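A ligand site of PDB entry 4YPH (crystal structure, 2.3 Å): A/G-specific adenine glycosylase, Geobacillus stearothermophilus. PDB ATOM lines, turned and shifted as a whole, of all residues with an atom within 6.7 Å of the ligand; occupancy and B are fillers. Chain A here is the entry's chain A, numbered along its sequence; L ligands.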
ATOM      1  N   ARG A 152       5.258  22.884  -7.239  1.00  0.00           N
ATOM      2  CA  ARG A 152       5.564  24.259  -6.867  1.00  0.00           C
ATOM      3  C   ARG A 152       7.081  24.470  -6.875  1.00  0.00           C
ATOM      4  O   ARG A 152       7.586  25.384  -7.520  1.00  0.00           O
ATOM      5  CB  ARG A 152       4.964  24.592  -5.477  1.00  0.00           C
ATOM      6  CG  ARG A 152       4.997  26.067  -5.082  1.00  0.00           C
ATOM      7  CD  ARG A 152       4.086  26.342  -3.871  1.00  0.00           C
ATOM      8  NE  ARG A 152       4.542  25.528  -2.745  1.00  0.00           N
ATOM      9  CZ  ARG A 152       3.906  24.457  -2.284  1.00  0.00           C
ATOM     10  NH1 ARG A 152       2.749  24.077  -2.820  1.00  0.00           N
ATOM     11  NH2 ARG A 152       4.428  23.790  -1.267  1.00  0.00           N
ATOM     12  N   VAL A 153       7.807  23.598  -6.191  1.00  0.00           N
ATOM     13  CA  VAL A 153       9.240  23.765  -6.097  1.00  0.00           C
ATOM     14  C   VAL A 153       9.865  23.809  -7.479  1.00  0.00           C
ATOM     15  O   VAL A 153      10.642  24.705  -7.779  1.00  0.00           O
ATOM     16  CB  VAL A 153       9.882  22.626  -5.299  1.00  0.00           C
ATOM     17  CG1 VAL A 153      11.412  22.711  -5.428  1.00  0.00           C
ATOM     18  CG2 VAL A 153       9.445  22.679  -3.853  1.00  0.00           C
ATOM     19  N   ARG A 156       9.156  26.777  -9.528  1.00  0.00           N
ATOM     20  CA  ARG A 156       9.966  27.934  -9.204  1.00  0.00           C
ATOM     21  C   ARG A 156      11.428  27.747  -9.605  1.00  0.00           C
ATOM     22  O   ARG A 156      12.090  28.666 -10.100  1.00  0.00           O
ATOM     23  CB  ARG A 156       9.856  28.275  -7.710  1.00  0.00           C
ATOM     24  CG  ARG A 156       8.576  29.017  -7.367  1.00  0.00           C
ATOM     25  CD  ARG A 156       8.006  28.571  -6.028  1.00  0.00           C
ATOM     26  NE  ARG A 156       6.768  29.276  -5.700  1.00  0.00           N
ATOM     27  CZ  ARG A 156       6.254  29.367  -4.469  1.00  0.00           C
ATOM     28  NH1 ARG A 156       6.883  28.817  -3.432  1.00  0.00           N
ATOM     29  NH2 ARG A 156       5.118  30.028  -4.271  1.00  0.00           N
ATOM     30  N   LEU A 157      11.957  26.551  -9.414  1.00  0.00           N
ATOM     31  CA  LEU A 157      13.375  26.365  -9.616  1.00  0.00           C
ATOM     32  C   LEU A 157      13.693  26.626 -11.076  1.00  0.00           C
ATOM     33  O   LEU A 157      14.664  27.295 -11.400  1.00  0.00           O
ATOM     34  CB  LEU A 157      13.805  24.958  -9.190  1.00  0.00           C
ATOM     35  CG  LEU A 157      14.102  24.782  -7.697  1.00  0.00           C
ATOM     36  CD1 LEU A 157      14.352  23.327  -7.336  1.00  0.00           C
ATOM     37  CD2 LEU A 157      15.273  25.626  -7.238  1.00  0.00           C
ATOM     38  N   LEU A 196      10.829  20.412   1.318  1.00  0.00           N
ATOM     39  CA  LEU A 196      11.204  21.760   0.959  1.00  0.00           C
ATOM     40  C   LEU A 196       9.958  22.535   0.589  1.00  0.00           C
ATOM     41  O   LEU A 196       9.797  23.692   0.945  1.00  0.00           O
ATOM     42  CB  LEU A 196      12.216  21.765  -0.186  1.00  0.00           C
ATOM     43  CG  LEU A 196      12.782  23.123  -0.569  1.00  0.00           C
ATOM     44  CD1 LEU A 196      13.796  23.624   0.473  1.00  0.00           C
ATOM     45  CD2 LEU A 196      13.402  23.143  -1.978  1.00  0.00           C
ATOM     46  N   VAL A 200       9.607  25.420   3.436  1.00  0.00           N
ATOM     47  CA  VAL A 200      10.342  26.587   2.936  1.00  0.00           C
ATOM     48  C   VAL A 200       9.647  27.229   1.714  1.00  0.00           C
ATOM     49  O   VAL A 200       9.199  28.370   1.750  1.00  0.00           O
ATOM     50  CB  VAL A 200      11.815  26.205   2.537  1.00  0.00           C
ATOM     51  CG1 VAL A 200      12.555  27.402   1.985  1.00  0.00           C
ATOM     52  CG2 VAL A 200      12.570  25.636   3.741  1.00  0.00           C
ATOM     53  N   CYS A 201       9.588  26.452   0.634  1.00  0.00           N
ATOM     54  CA  CYS A 201       9.078  26.904  -0.646  1.00  0.00           C
ATOM     55  C   CYS A 201       7.559  26.815  -0.689  1.00  0.00           C
ATOM     56  O   CYS A 201       6.973  26.038  -1.433  1.00  0.00           O
ATOM     57  CB  CYS A 201       9.698  26.068  -1.768  1.00  0.00           C
ATOM     58  SG  CYS A 201       9.301  26.661  -3.423  1.00  0.00           S
ATOM     59  N   THR A 202       6.918  27.617   0.148  1.00  0.00           N
ATOM     60  CA  THR A 202       5.500  27.466   0.457  1.00  0.00           C
ATOM     61  C   THR A 202       4.647  28.203  -0.560  1.00  0.00           C
ATOM     62  O   THR A 202       5.140  29.113  -1.231  1.00  0.00           O
ATOM     63  CB  THR A 202       5.211  28.005   1.893  1.00  0.00           C
ATOM     64  OG1 THR A 202       5.803  29.315   2.062  1.00  0.00           O
ATOM     65  CG2 THR A 202       5.840  27.054   2.914  1.00  0.00           C
ATOM     66  N   PRO A 206       7.177  32.283   0.017  1.00  0.00           N
ATOM     67  CA  PRO A 206       8.199  31.266   0.250  1.00  0.00           C
ATOM     68  C   PRO A 206       9.441  31.854   0.949  1.00  0.00           C
ATOM     69  O   PRO A 206       9.714  33.033   0.775  1.00  0.00           O
ATOM     70  CB  PRO A 206       8.512  30.758  -1.169  1.00  0.00           C
ATOM     71  CG  PRO A 206       8.087  31.893  -2.101  1.00  0.00           C
ATOM     72  CD  PRO A 206       6.913  32.517  -1.423  1.00  0.00           C
ATOM     73  N   SER A 207      10.151  31.051   1.719  1.00  0.00           N
ATOM     74  CA  SER A 207      11.217  31.591   2.564  1.00  0.00           C
ATOM     75  C   SER A 207      12.549  31.522   1.872  1.00  0.00           C
ATOM     76  O   SER A 207      13.512  30.918   2.359  1.00  0.00           O
ATOM     77  CB  SER A 207      11.279  30.842   3.899  1.00  0.00           C
ATOM     78  OG  SER A 207      10.054  31.014   4.592  1.00  0.00           O
ATOM     79  N   CYS A 208      12.567  32.173   0.705  1.00  0.00           N
ATOM     80  CA  CYS A 208      13.676  32.172  -0.217  1.00  0.00           C
ATOM     81  C   CYS A 208      15.028  32.524   0.422  1.00  0.00           C
ATOM     82  O   CYS A 208      16.042  31.926   0.071  1.00  0.00           O
ATOM     83  CB  CYS A 208      13.384  33.161  -1.368  1.00  0.00           C
ATOM     84  SG  CYS A 208      11.806  32.918  -2.285  1.00  0.00           S
ATOM     85  N   LEU A 209      15.025  33.489   1.335  1.00  0.00           N
ATOM     86  CA  LEU A 209      16.279  33.982   1.921  1.00  0.00           C
ATOM     87  C   LEU A 209      16.907  32.862   2.756  1.00  0.00           C
ATOM     88  O   LEU A 209      18.093  32.829   2.974  1.00  0.00           O
ATOM     89  CB  LEU A 209      16.013  35.226   2.781  1.00  0.00           C
ATOM     90  CG  LEU A 209      15.194  36.327   2.072  1.00  0.00           C
ATOM     91  CD1 LEU A 209      14.808  37.462   3.006  1.00  0.00           C
ATOM     92  CD2 LEU A 209      15.909  36.921   0.877  1.00  0.00           C
ATOM     93  N   LEU A 210      16.059  31.936   3.184  1.00  0.00           N
ATOM     94  CA  LEU A 210      16.476  30.767   3.936  1.00  0.00           C
ATOM     95  C   LEU A 210      16.600  29.498   3.090  1.00  0.00           C
ATOM     96  O   LEU A 210      17.066  28.466   3.575  1.00  0.00           O
ATOM     97  CB  LEU A 210      15.495  30.522   5.069  1.00  0.00           C
ATOM     98  CG  LEU A 210      15.464  31.656   6.104  1.00  0.00           C
ATOM     99  CD1 LEU A 210      14.608  31.302   7.262  1.00  0.00           C
ATOM    100  CD2 LEU A 210      16.873  31.996   6.550  1.00  0.00           C
ATOM    101  N   CYS A 211      16.191  29.534   1.827  1.00  0.00           N
ATOM    102  CA  CYS A 211      16.160  28.286   1.073  1.00  0.00           C
ATOM    103  C   CYS A 211      17.546  27.689   0.737  1.00  0.00           C
ATOM    104  O   CYS A 211      18.447  28.364   0.255  1.00  0.00           O
ATOM    105  CB  CYS A 211      15.372  28.452  -0.222  1.00  0.00           C
ATOM    106  SG  CYS A 211      15.427  26.928  -1.198  1.00  0.00           S
ATOM    107  N   PRO A 212      17.713  26.382   0.980  1.00  0.00           N
ATOM    108  CA  PRO A 212      19.010  25.725   0.717  1.00  0.00           C
ATOM    109  C   PRO A 212      19.370  25.650  -0.767  1.00  0.00           C
ATOM    110  O   PRO A 212      20.516  25.390  -1.054  1.00  0.00           O
ATOM    111  CB  PRO A 212      18.810  24.316   1.271  1.00  0.00           C
ATOM    112  CG  PRO A 212      17.290  24.110   1.146  1.00  0.00           C
ATOM    113  CD  PRO A 212      16.725  25.449   1.519  1.00  0.00           C
ATOM    114  N   VAL A 213      18.414  25.835  -1.674  1.00  0.00           N
ATOM    115  CA  VAL A 213      18.722  25.704  -3.103  1.00  0.00           C
ATOM    116  C   VAL A 213      18.469  27.014  -3.842  1.00  0.00           C
ATOM    117  O   VAL A 213      18.363  27.041  -5.068  1.00  0.00           O
ATOM    118  CB  VAL A 213      17.930  24.542  -3.759  1.00  0.00           C
ATOM    119  CG1 VAL A 213      18.284  23.234  -3.068  1.00  0.00           C
ATOM    120  CG2 VAL A 213      16.442  24.780  -3.688  1.00  0.00           C
ATOM    121  N   GLN A 214      18.410  28.099  -3.077  1.00  0.00           N
ATOM    122  CA  GLN A 214      18.208  29.416  -3.652  1.00  0.00           C
ATOM    123  C   GLN A 214      19.147  29.727  -4.831  1.00  0.00           C
ATOM    124  O   GLN A 214      18.731  30.303  -5.850  1.00  0.00           O
ATOM    125  CB  GLN A 214      18.372  30.480  -2.575  1.00  0.00           C
ATOM    126  CG  GLN A 214      18.226  31.896  -3.090  1.00  0.00           C
ATOM    127  CD  GLN A 214      19.127  32.900  -2.351  1.00  0.00           C
ATOM    128  OE1 GLN A 214      20.164  33.329  -2.880  1.00  0.00           O
ATOM    129  NE2 GLN A 214      18.732  33.282  -1.142  1.00  0.00           N
ATOM    130  N   ALA A 215      20.405  29.356  -4.695  1.00  0.00           N
ATOM    131  CA  ALA A 215      21.380  29.678  -5.748  1.00  0.00           C
ATOM    132  C   ALA A 215      21.020  29.013  -7.073  1.00  0.00           C
ATOM    133  O   ALA A 215      21.466  29.466  -8.121  1.00  0.00           O
ATOM    134  CB  ALA A 215      22.758  29.289  -5.332  1.00  0.00           C
ATOM    135  N   TYR A 216      20.197  27.962  -7.017  1.00  0.00           N
ATOM    136  CA  TYR A 216      19.802  27.251  -8.229  1.00  0.00           C
ATOM    137  C   TYR A 216      18.490  27.768  -8.796  1.00  0.00           C
ATOM    138  O   TYR A 216      18.112  27.421  -9.914  1.00  0.00           O
ATOM    139  CB  TYR A 216      19.671  25.760  -7.962  1.00  0.00           C
ATOM    140  CG  TYR A 216      20.858  25.141  -7.287  1.00  0.00           C
ATOM    141  CD1 TYR A 216      20.881  24.995  -5.926  1.00  0.00           C
ATOM    142  CD2 TYR A 216      21.965  24.707  -8.019  1.00  0.00           C
ATOM    143  CE1 TYR A 216      21.959  24.452  -5.279  1.00  0.00           C
ATOM    144  CE2 TYR A 216      23.056  24.150  -7.386  1.00  0.00           C
ATOM    145  CZ  TYR A 216      23.039  24.022  -5.998  1.00  0.00           C
ATOM    146  OH  TYR A 216      24.077  23.475  -5.287  1.00  0.00           O
ATOM    147  N   CYS A 217      17.796  28.600  -8.040  1.00  0.00           N
ATOM    148  CA  CYS A 217      16.428  28.927  -8.406  1.00  0.00           C
ATOM    149  C   CYS A 217      16.220  30.136  -9.329  1.00  0.00           C
ATOM    150  O   CYS A 217      16.629  31.254  -9.023  1.00  0.00           O
ATOM    151  CB  CYS A 217      15.613  29.144  -7.132  1.00  0.00           C
ATOM    152  SG  CYS A 217      13.935  29.662  -7.549  1.00  0.00           S
ATOM    153  N   GLN A 218      15.518  29.914 -10.427  1.00  0.00           N
ATOM    154  CA  GLN A 218      15.296  30.968 -11.420  1.00  0.00           C
ATOM    155  C   GLN A 218      14.211  31.942 -11.004  1.00  0.00           C
ATOM    156  O   GLN A 218      14.319  33.137 -11.281  1.00  0.00           O
ATOM    157  CB  GLN A 218      14.921  30.373 -12.759  1.00  0.00           C
ATOM    158  CG  GLN A 218      16.085  29.983 -13.603  1.00  0.00           C
ATOM    159  CD  GLN A 218      15.650  29.225 -14.811  1.00  0.00           C
ATOM    160  OE1 GLN A 218      15.668  27.986 -14.808  1.00  0.00           O
ATOM    161  NE2 GLN A 218      15.210  29.943 -15.840  1.00  0.00           N
ATOM    162  N   ALA A 219      13.146  31.427 -10.404  1.00  0.00           N
ATOM    163  CA  ALA A 219      12.055  32.315 -10.016  1.00  0.00           C
ATOM    164  C   ALA A 219      12.565  33.347  -8.996  1.00  0.00           C
ATOM    165  O   ALA A 219      12.183  34.512  -9.017  1.00  0.00           O
ATOM    166  CB  ALA A 219      10.885  31.527  -9.447  1.00  0.00           C
ATOM    167  N   PHE A 220      13.442  32.899  -8.113  1.00  0.00           N
ATOM    168  CA  PHE A 220      14.010  33.795  -7.134  1.00  0.00           C
ATOM    169  C   PHE A 220      14.875  34.825  -7.864  1.00  0.00           C
ATOM    170  O   PHE A 220      14.831  36.013  -7.556  1.00  0.00           O
ATOM    171  CB  PHE A 220      14.839  33.045  -6.092  1.00  0.00           C
ATOM    172  CG  PHE A 220      15.547  33.947  -5.123  1.00  0.00           C
ATOM    173  CD1 PHE A 220      14.834  34.576  -4.104  1.00  0.00           C
ATOM    174  CD2 PHE A 220      16.902  34.203  -5.241  1.00  0.00           C
ATOM    175  CE1 PHE A 220      15.460  35.423  -3.200  1.00  0.00           C
ATOM    176  CE2 PHE A 220      17.555  35.054  -4.350  1.00  0.00           C
ATOM    177  CZ  PHE A 220      16.835  35.657  -3.313  1.00  0.00           C
ATOM    178  N   ALA A 225       8.974  34.260  -7.462  1.00  0.00           N
ATOM    179  CA  ALA A 225       8.667  33.068  -6.634  1.00  0.00           C
ATOM    180  C   ALA A 225       7.190  32.929  -6.288  1.00  0.00           C
ATOM    181  O   ALA A 225       6.611  31.850  -6.420  1.00  0.00           O
ATOM    182  CB  ALA A 225       9.480  33.100  -5.359  1.00  0.00           C
ATOM    183  N   GLU A 226       6.591  34.024  -5.873  1.00  0.00           N
ATOM    184  CA  GLU A 226       5.217  34.028  -5.374  1.00  0.00           C
ATOM    185  C   GLU A 226       4.169  33.856  -6.473  1.00  0.00           C
ATOM    186  O   GLU A 226       3.036  33.491  -6.186  1.00  0.00           O
ATOM    187  CB  GLU A 226       4.935  35.333  -4.626  1.00  0.00           C
ATOM    188  CG  GLU A 226       4.889  35.251  -3.120  1.00  0.00           C
ATOM    189  CD  GLU A 226       5.105  36.616  -2.471  1.00  0.00           C
ATOM    190  OE1 GLU A 226       4.611  36.837  -1.347  1.00  0.00           O
ATOM    191  OE2 GLU A 226       5.772  37.476  -3.105  1.00  0.00           O
HETATM  192 FE1  LIG L   1      12.329  30.612  -2.971  1.00  0.00          FE
HETATM  193 FE2  LIG L   1      11.221  28.026  -3.629  1.00  0.00          FE
HETATM  194 FE3  LIG L   1      13.876  28.246  -2.544  1.00  0.00          FE
HETATM  195 FE4  LIG L   1      13.369  29.076  -5.243  1.00  0.00          FE
HETATM  196  S1  LIG L   1      13.092  27.150  -4.284  1.00  0.00           S
HETATM  197  S2  LIG L   1      14.370  30.087  -3.581  1.00  0.00           S
HETATM  198  S3  LIG L   1      11.384  29.834  -4.773  1.00  0.00           S
HETATM  199  S4  LIG L   1      11.925  28.881  -1.748  1.00  0.00           S
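Residues that only touch the ligand: Arg 156, Leu 157, Pro 206, Gln 214, Phe 220 and Ala 225.
Of the 25 residues printed, 10 come within 4 Å of the ligand.
O of Leu 196 sits at hydrogen-bond distance from N of Cys 201 (2.8 Å).
SG of Cys 211 lies close to N of Gln 214 (3.7 Å).
N of Val 213 lies close to SG of Cys 211.
The side-chain sulfur (SG) of Cys 217 lies close to the backbone carbonyl oxygen (O) of Arg 156.
The side-chain sulfur of Cys 217 sits close to the backbone NH of Phe 220 (3.3 Å).
SG of Cys 217 sits close to N of Ala 219 (3.4 Å).
The guanidinium group (NE) of Arg 156 sits at hydrogen-bond distance from the backbone carbonyl oxygen (O) of Ala 225, at 2.7 Å.
The backbone carbonyl oxygen (O) of Arg 156 sits at hydrogen-bond distance from the backbone NH (N) of Ala 219 (3.0 Å).
SG of Cys 201 is bound to FE2 of the ligand.
SG of Cys 211 is bound to FE3 of the ligand, 2.4 Å away.
The side-chain sulfur of Cys 217 binds an iron atom (FE4) of the ligand (2.4 Å).
An iron atom (FE1) of the ligand is bound by the side-chain sulfur (SG) of Cys 208 (2.5 Å).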
